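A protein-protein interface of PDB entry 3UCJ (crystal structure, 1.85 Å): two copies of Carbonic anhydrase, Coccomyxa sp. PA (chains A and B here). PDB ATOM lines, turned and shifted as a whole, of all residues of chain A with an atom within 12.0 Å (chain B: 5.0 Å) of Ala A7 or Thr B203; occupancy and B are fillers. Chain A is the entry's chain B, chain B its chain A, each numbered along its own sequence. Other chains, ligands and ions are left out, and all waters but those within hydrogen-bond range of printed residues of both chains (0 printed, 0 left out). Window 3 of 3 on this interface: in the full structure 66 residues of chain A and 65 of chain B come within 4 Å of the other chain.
No position is printed for both chains.
A ring nitrogen (ND1) of His B97 lies within hydrogen-bond range of the side-chain hydroxyl (OG) of Ser B182, 2.8 Å away.
The side-chain hydroxyl of Ser B182 sits at hydrogen-bond distance from a ring nitrogen (NE2) of His B184.
OG1 of Thr B203 lies within hydrogen-bond range of OD1 of Asp B207 (2.7 Å).
Of chain B, only Ser B182 (3.7 Å), His B184 (3.2 Å), Pro B201 (3.4 Å) and Thr B203 (3.9 Å) come within 4 Å of Ala A7.
No residue of chain A comes within 4 Å of Ile B202.
No residue of chain A comes within 4 Å of Gly B204.
No residue of chain A comes within 4 Å of Asp B207.
Printed residues of chain B within 4 Å of Leu A9: His B184 (3.5 Å).
Printed residues of chain B within 4 Å of Thr A6: His B97 (3.5 Å).
Of the printed residues of chain A, His B97 touches Thr A6 (3.5 Å).
Printed residues of chain A within 4 Å of His B184: Ala A7 (3.2 Å) and Leu A9 (3.5 Å).
Ser A10 touches none of the printed residues of chain B.
The nearest residue of chain B that does not touch Ala A7 is His B97 (4.1 Å).
The nearest printed residue of chain B that does not touch Leu A9 is Pro B201 (4.8 Å).
Hydrophobic or aromatic side chains of chain A that line the printed part of chain B: Ala A7 and Leu A9.
Among the printed residues, 6 pairs touch across the chains.
Among the printed residues, pairs that only touch across the chains: Ala A7 with His B184 (3.2 Å), Ala A7 with Pro B201 (3.4 Å), Leu A9 with His B184 (3.5 Å), Thr A6 with His B97 (3.5 Å), Ala A7 with Ser B182 (3.7 Å) and Ala A7 with Thr B203 (3.9 Å).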
ATOM      1  N   THR A   6      32.463  -8.022 -31.118  1.00  0.00           N
ATOM      2  CA  THR A   6      32.623  -6.754 -30.312  1.00  0.00           C
ATOM      3  C   THR A   6      31.709  -6.832 -29.057  1.00  0.00           C
ATOM      4  O   THR A   6      32.224  -6.890 -27.896  1.00  0.00           O
ATOM      5  CB  THR A   6      32.413  -5.362 -31.149  1.00  0.00           C
ATOM      6  OG1 THR A   6      31.555  -5.560 -32.292  1.00  0.00           O
ATOM      7  CG2 THR A   6      33.783  -4.724 -31.607  1.00  0.00           C
ATOM      8  N   ALA A   7      30.377  -6.879 -29.275  1.00  0.00           N
ATOM      9  CA  ALA A   7      29.458  -7.010 -28.131  1.00  0.00           C
ATOM     10  C   ALA A   7      29.082  -8.449 -27.671  1.00  0.00           C
ATOM     11  O   ALA A   7      28.341  -8.619 -26.682  1.00  0.00           O
ATOM     12  CB  ALA A   7      28.216  -6.106 -28.307  1.00  0.00           C
ATOM     13  N   ASP A   8      29.585  -9.487 -28.345  1.00  0.00           N
ATOM     14  CA  ASP A   8      29.243 -10.844 -27.940  1.00  0.00           C
ATOM     15  C   ASP A   8      29.752 -11.137 -26.507  1.00  0.00           C
ATOM     16  O   ASP A   8      30.828 -10.673 -26.151  1.00  0.00           O
ATOM     17  CB  ASP A   8      29.810 -11.857 -28.958  1.00  0.00           C
ATOM     18  CG  ASP A   8      29.634 -13.280 -28.510  1.00  0.00           C
ATOM     19  OD1 ASP A   8      28.610 -13.899 -28.857  1.00  0.00           O
ATOM     20  OD2 ASP A   8      30.508 -13.781 -27.777  1.00  0.00           O
ATOM     21  N   LEU A   9      28.978 -11.879 -25.682  1.00  0.00           N
ATOM     22  CA  LEU A   9      29.312 -12.158 -24.241  1.00  0.00           C
ATOM     23  C   LEU A   9      29.983 -13.492 -23.923  1.00  0.00           C
ATOM     24  O   LEU A   9      30.252 -13.765 -22.756  1.00  0.00           O
ATOM     25  CB  LEU A   9      28.034 -12.165 -23.345  1.00  0.00           C
ATOM     26  CG  LEU A   9      27.238 -10.935 -22.881  1.00  0.00           C
ATOM     27  CD1 LEU A   9      26.159 -11.340 -21.753  1.00  0.00           C
ATOM     28  CD2 LEU A   9      28.160  -9.805 -22.468  1.00  0.00           C
ATOM     29  N   SER A  10      30.184 -14.373 -24.914  1.00  0.00           N
ATOM     30  CA  SER A  10      30.707 -15.753 -24.616  1.00  0.00           C
ATOM     31  C   SER A  10      31.996 -15.743 -23.800  1.00  0.00           C
ATOM     32  O   SER A  10      32.139 -16.519 -22.846  1.00  0.00           O
ATOM     33  CB  SER A  10      30.910 -16.597 -25.901  1.00  0.00           C
ATOM     34  OG  SER A  10      30.072 -16.143 -26.956  1.00  0.00           O
ATOM     35  N   PRO A  11      32.928 -14.842 -24.136  1.00  0.00           N
ATOM     36  CA  PRO A  11      34.145 -14.809 -23.330  1.00  0.00           C
ATOM     37  C   PRO A  11      33.864 -14.546 -21.818  1.00  0.00           C
ATOM     38  O   PRO A  11      34.433 -15.217 -20.944  1.00  0.00           O
ATOM     39  CB  PRO A  11      34.960 -13.635 -23.970  1.00  0.00           C
ATOM     40  CG  PRO A  11      34.478 -13.532 -25.335  1.00  0.00           C
ATOM     41  CD  PRO A  11      32.997 -13.905 -25.277  1.00  0.00           C
ATOM     42  N   LEU A  12      32.992 -13.559 -21.515  1.00  0.00           N
ATOM     43  CA  LEU A  12      32.579 -13.317 -20.134  1.00  0.00           C
ATOM     44  C   LEU A  12      31.900 -14.537 -19.551  1.00  0.00           C
ATOM     45  O   LEU A  12      32.203 -14.966 -18.431  1.00  0.00           O
ATOM     46  CB  LEU A  12      31.606 -12.132 -20.085  1.00  0.00           C
ATOM     47  CG  LEU A  12      32.091 -10.773 -19.616  1.00  0.00           C
ATOM     48  CD1 LEU A  12      30.841  -9.863 -19.487  1.00  0.00           C
ATOM     49  CD2 LEU A  12      32.809 -10.882 -18.300  1.00  0.00           C
ATOM     50  N   LEU A  13      30.943 -15.105 -20.282  1.00  0.00           N
ATOM     51  CA  LEU A  13      30.220 -16.301 -19.767  1.00  0.00           C
ATOM     52  C   LEU A  13      31.165 -17.456 -19.465  1.00  0.00           C
ATOM     53  O   LEU A  13      31.074 -18.155 -18.426  1.00  0.00           O
ATOM     54  CB  LEU A  13      29.150 -16.708 -20.771  1.00  0.00           C
ATOM     55  CG  LEU A  13      28.052 -15.656 -20.962  1.00  0.00           C
ATOM     56  CD1 LEU A  13      27.107 -16.091 -22.088  1.00  0.00           C
ATOM     57  CD2 LEU A  13      27.323 -15.519 -19.622  1.00  0.00           C
ATOM     58  N   GLU A  14      32.132 -17.619 -20.357  1.00  0.00           N
ATOM     59  CA  GLU A  14      33.149 -18.661 -20.158  1.00  0.00           C
ATOM     60  C   GLU A  14      34.034 -18.387 -18.941  1.00  0.00           C
ATOM     61  O   GLU A  14      34.370 -19.294 -18.188  1.00  0.00           O
ATOM     62  CB  GLU A  14      33.993 -18.884 -21.450  1.00  0.00           C
ATOM     63  CG  GLU A  14      34.844 -20.240 -21.431  1.00  0.00           C
ATOM     64  CD  GLU A  14      34.044 -21.519 -20.913  1.00  0.00           C
ATOM     65  OE1 GLU A  14      32.942 -21.847 -21.454  1.00  0.00           O
ATOM     66  OE2 GLU A  14      34.505 -22.194 -19.929  1.00  0.00           O
ATOM     67  N   HIS B  97      29.956  -1.600 -22.598  1.00  0.00           N
ATOM     68  CA  HIS B  97      28.932  -2.626 -22.362  1.00  0.00           C
ATOM     69  C   HIS B  97      28.248  -2.374 -20.969  1.00  0.00           C
ATOM     70  O   HIS B  97      28.950  -2.218 -19.963  1.00  0.00           O
ATOM     71  CB  HIS B  97      29.560  -4.013 -22.292  1.00  0.00           C
ATOM     72  CG  HIS B  97      30.563  -4.289 -23.380  1.00  0.00           C
ATOM     73  ND1 HIS B  97      30.225  -4.241 -24.728  1.00  0.00           N
ATOM     74  CD2 HIS B  97      31.900  -4.578 -23.324  1.00  0.00           C
ATOM     75  CE1 HIS B  97      31.310  -4.523 -25.453  1.00  0.00           C
ATOM     76  NE2 HIS B  97      32.332  -4.750 -24.632  1.00  0.00           N
ATOM     77  N   TRP B 175      23.733   6.768 -27.958  1.00  0.00           N
ATOM     78  CA  TRP B 175      23.381   6.232 -29.281  1.00  0.00           C
ATOM     79  C   TRP B 175      23.191   7.360 -30.324  1.00  0.00           C
ATOM     80  O   TRP B 175      23.664   7.224 -31.451  1.00  0.00           O
ATOM     81  CB  TRP B 175      22.165   5.307 -29.219  1.00  0.00           C
ATOM     82  CG  TRP B 175      22.423   3.965 -28.534  1.00  0.00           C
ATOM     83  CD1 TRP B 175      23.621   3.403 -28.255  1.00  0.00           C
ATOM     84  CD2 TRP B 175      21.415   3.004 -28.132  1.00  0.00           C
ATOM     85  NE1 TRP B 175      23.439   2.165 -27.697  1.00  0.00           N
ATOM     86  CE2 TRP B 175      22.089   1.897 -27.622  1.00  0.00           C
ATOM     87  CE3 TRP B 175      19.999   2.986 -28.210  1.00  0.00           C
ATOM     88  CZ2 TRP B 175      21.418   0.778 -27.110  1.00  0.00           C
ATOM     89  CZ3 TRP B 175      19.338   1.853 -27.760  1.00  0.00           C
ATOM     90  CH2 TRP B 175      20.038   0.773 -27.230  1.00  0.00           C
ATOM     91  N   LEU B 181      27.787   1.368 -27.679  1.00  0.00           N
ATOM     92  CA  LEU B 181      27.321   1.041 -26.297  1.00  0.00           C
ATOM     93  C   LEU B 181      26.389  -0.128 -26.465  1.00  0.00           C
ATOM     94  O   LEU B 181      25.419  -0.010 -27.142  1.00  0.00           O
ATOM     95  CB  LEU B 181      26.613   2.300 -25.745  1.00  0.00           C
ATOM     96  CG  LEU B 181      26.251   2.194 -24.210  1.00  0.00           C
ATOM     97  CD1 LEU B 181      27.416   1.815 -23.324  1.00  0.00           C
ATOM     98  CD2 LEU B 181      25.668   3.569 -23.916  1.00  0.00           C
ATOM     99  N   SER B 182      26.666  -1.237 -25.818  1.00  0.00           N
ATOM    100  CA  SER B 182      25.752  -2.348 -25.812  1.00  0.00           C
ATOM    101  C   SER B 182      25.112  -2.598 -24.391  1.00  0.00           C
ATOM    102  O   SER B 182      25.729  -2.289 -23.391  1.00  0.00           O
ATOM    103  CB  SER B 182      26.493  -3.606 -26.233  1.00  0.00           C
ATOM    104  OG  SER B 182      27.475  -4.028 -25.317  1.00  0.00           O
ATOM    105  N   HIS B 184      23.020  -5.633 -22.057  1.00  0.00           N
ATOM    106  CA  HIS B 184      22.853  -7.078 -21.882  1.00  0.00           C
ATOM    107  C   HIS B 184      21.944  -7.466 -20.759  1.00  0.00           C
ATOM    108  O   HIS B 184      22.186  -7.039 -19.594  1.00  0.00           O
ATOM    109  CB  HIS B 184      24.220  -7.675 -21.631  1.00  0.00           C
ATOM    110  CG  HIS B 184      25.234  -7.237 -22.656  1.00  0.00           C
ATOM    111  ND1 HIS B 184      25.498  -7.965 -23.804  1.00  0.00           N
ATOM    112  CD2 HIS B 184      25.955  -6.089 -22.760  1.00  0.00           C
ATOM    113  CE1 HIS B 184      26.398  -7.326 -24.532  1.00  0.00           C
ATOM    114  NE2 HIS B 184      26.682  -6.178 -23.935  1.00  0.00           N
ATOM    115  N   PRO B 201      22.794  -9.326 -27.084  1.00  0.00           N
ATOM    116  CA  PRO B 201      23.248  -7.942 -27.000  1.00  0.00           C
ATOM    117  C   PRO B 201      22.369  -6.980 -27.783  1.00  0.00           C
ATOM    118  O   PRO B 201      21.901  -7.332 -28.902  1.00  0.00           O
ATOM    119  CB  PRO B 201      24.654  -8.019 -27.611  1.00  0.00           C
ATOM    120  CG  PRO B 201      25.128  -9.403 -27.267  1.00  0.00           C
ATOM    121  CD  PRO B 201      23.912 -10.243 -27.460  1.00  0.00           C
ATOM    122  N   ILE B 202      22.142  -5.759 -27.233  1.00  0.00           N
ATOM    123  CA  ILE B 202      21.386  -4.701 -27.863  1.00  0.00           C
ATOM    124  C   ILE B 202      22.364  -3.578 -28.051  1.00  0.00           C
ATOM    125  O   ILE B 202      22.905  -3.053 -27.045  1.00  0.00           O
ATOM    126  CB  ILE B 202      20.176  -4.204 -26.983  1.00  0.00           C
ATOM    127  CG1 ILE B 202      19.132  -5.339 -26.879  1.00  0.00           C
ATOM    128  CG2 ILE B 202      19.512  -2.962 -27.643  1.00  0.00           C
ATOM    129  CD1 ILE B 202      18.140  -5.297 -25.769  1.00  0.00           C
ATOM    130  N   THR B 203      22.689  -3.251 -29.320  1.00  0.00           N
ATOM    131  CA  THR B 203      23.749  -2.303 -29.578  1.00  0.00           C
ATOM    132  C   THR B 203      23.134  -1.074 -30.097  1.00  0.00           C
ATOM    133  O   THR B 203      23.840  -0.133 -30.403  1.00  0.00           O
ATOM    134  CB  THR B 203      24.788  -2.811 -30.692  1.00  0.00           C
ATOM    135  OG1 THR B 203      24.027  -3.039 -31.868  1.00  0.00           O
ATOM    136  CG2 THR B 203      25.498  -4.054 -30.271  1.00  0.00           C
ATOM    137  N   GLY B 204      21.819  -1.028 -30.237  1.00  0.00           N
ATOM    138  CA  GLY B 204      21.152   0.183 -30.700  1.00  0.00           C
ATOM    139  C   GLY B 204      19.688  -0.075 -30.957  1.00  0.00           C
ATOM    140  O   GLY B 204      19.199  -1.155 -30.621  1.00  0.00           O
ATOM    141  N   MET B 205      19.005   0.903 -31.533  1.00  0.00           N
ATOM    142  CA  MET B 205      17.570   0.855 -31.717  1.00  0.00           C
ATOM    143  C   MET B 205      17.177  -0.336 -32.605  1.00  0.00           C
ATOM    144  O   MET B 205      16.263  -1.081 -32.265  1.00  0.00           O
ATOM    145  CB  MET B 205      17.035   2.138 -32.331  1.00  0.00           C
ATOM    146  CG  MET B 205      17.216   3.392 -31.431  1.00  0.00           C
ATOM    147  SD  MET B 205      16.098   3.176 -29.932  1.00  0.00           S
ATOM    148  CE  MET B 205      14.577   3.513 -30.673  1.00  0.00           C
ATOM    149  N   ASP B 207      18.614  -3.380 -32.890  1.00  0.00           N
ATOM    150  CA  ASP B 207      18.566  -4.597 -32.086  1.00  0.00           C
ATOM    151  C   ASP B 207      17.426  -4.587 -31.050  1.00  0.00           C
ATOM    152  O   ASP B 207      16.885  -5.627 -30.695  1.00  0.00           O
ATOM    153  CB  ASP B 207      19.826  -4.768 -31.258  1.00  0.00           C
ATOM    154  CG  ASP B 207      21.052  -5.053 -32.093  1.00  0.00           C
ATOM    155  OD1 ASP B 207      22.154  -4.911 -31.553  1.00  0.00           O
ATOM    156  OD2 ASP B 207      20.893  -5.443 -33.273  1.00  0.00           O
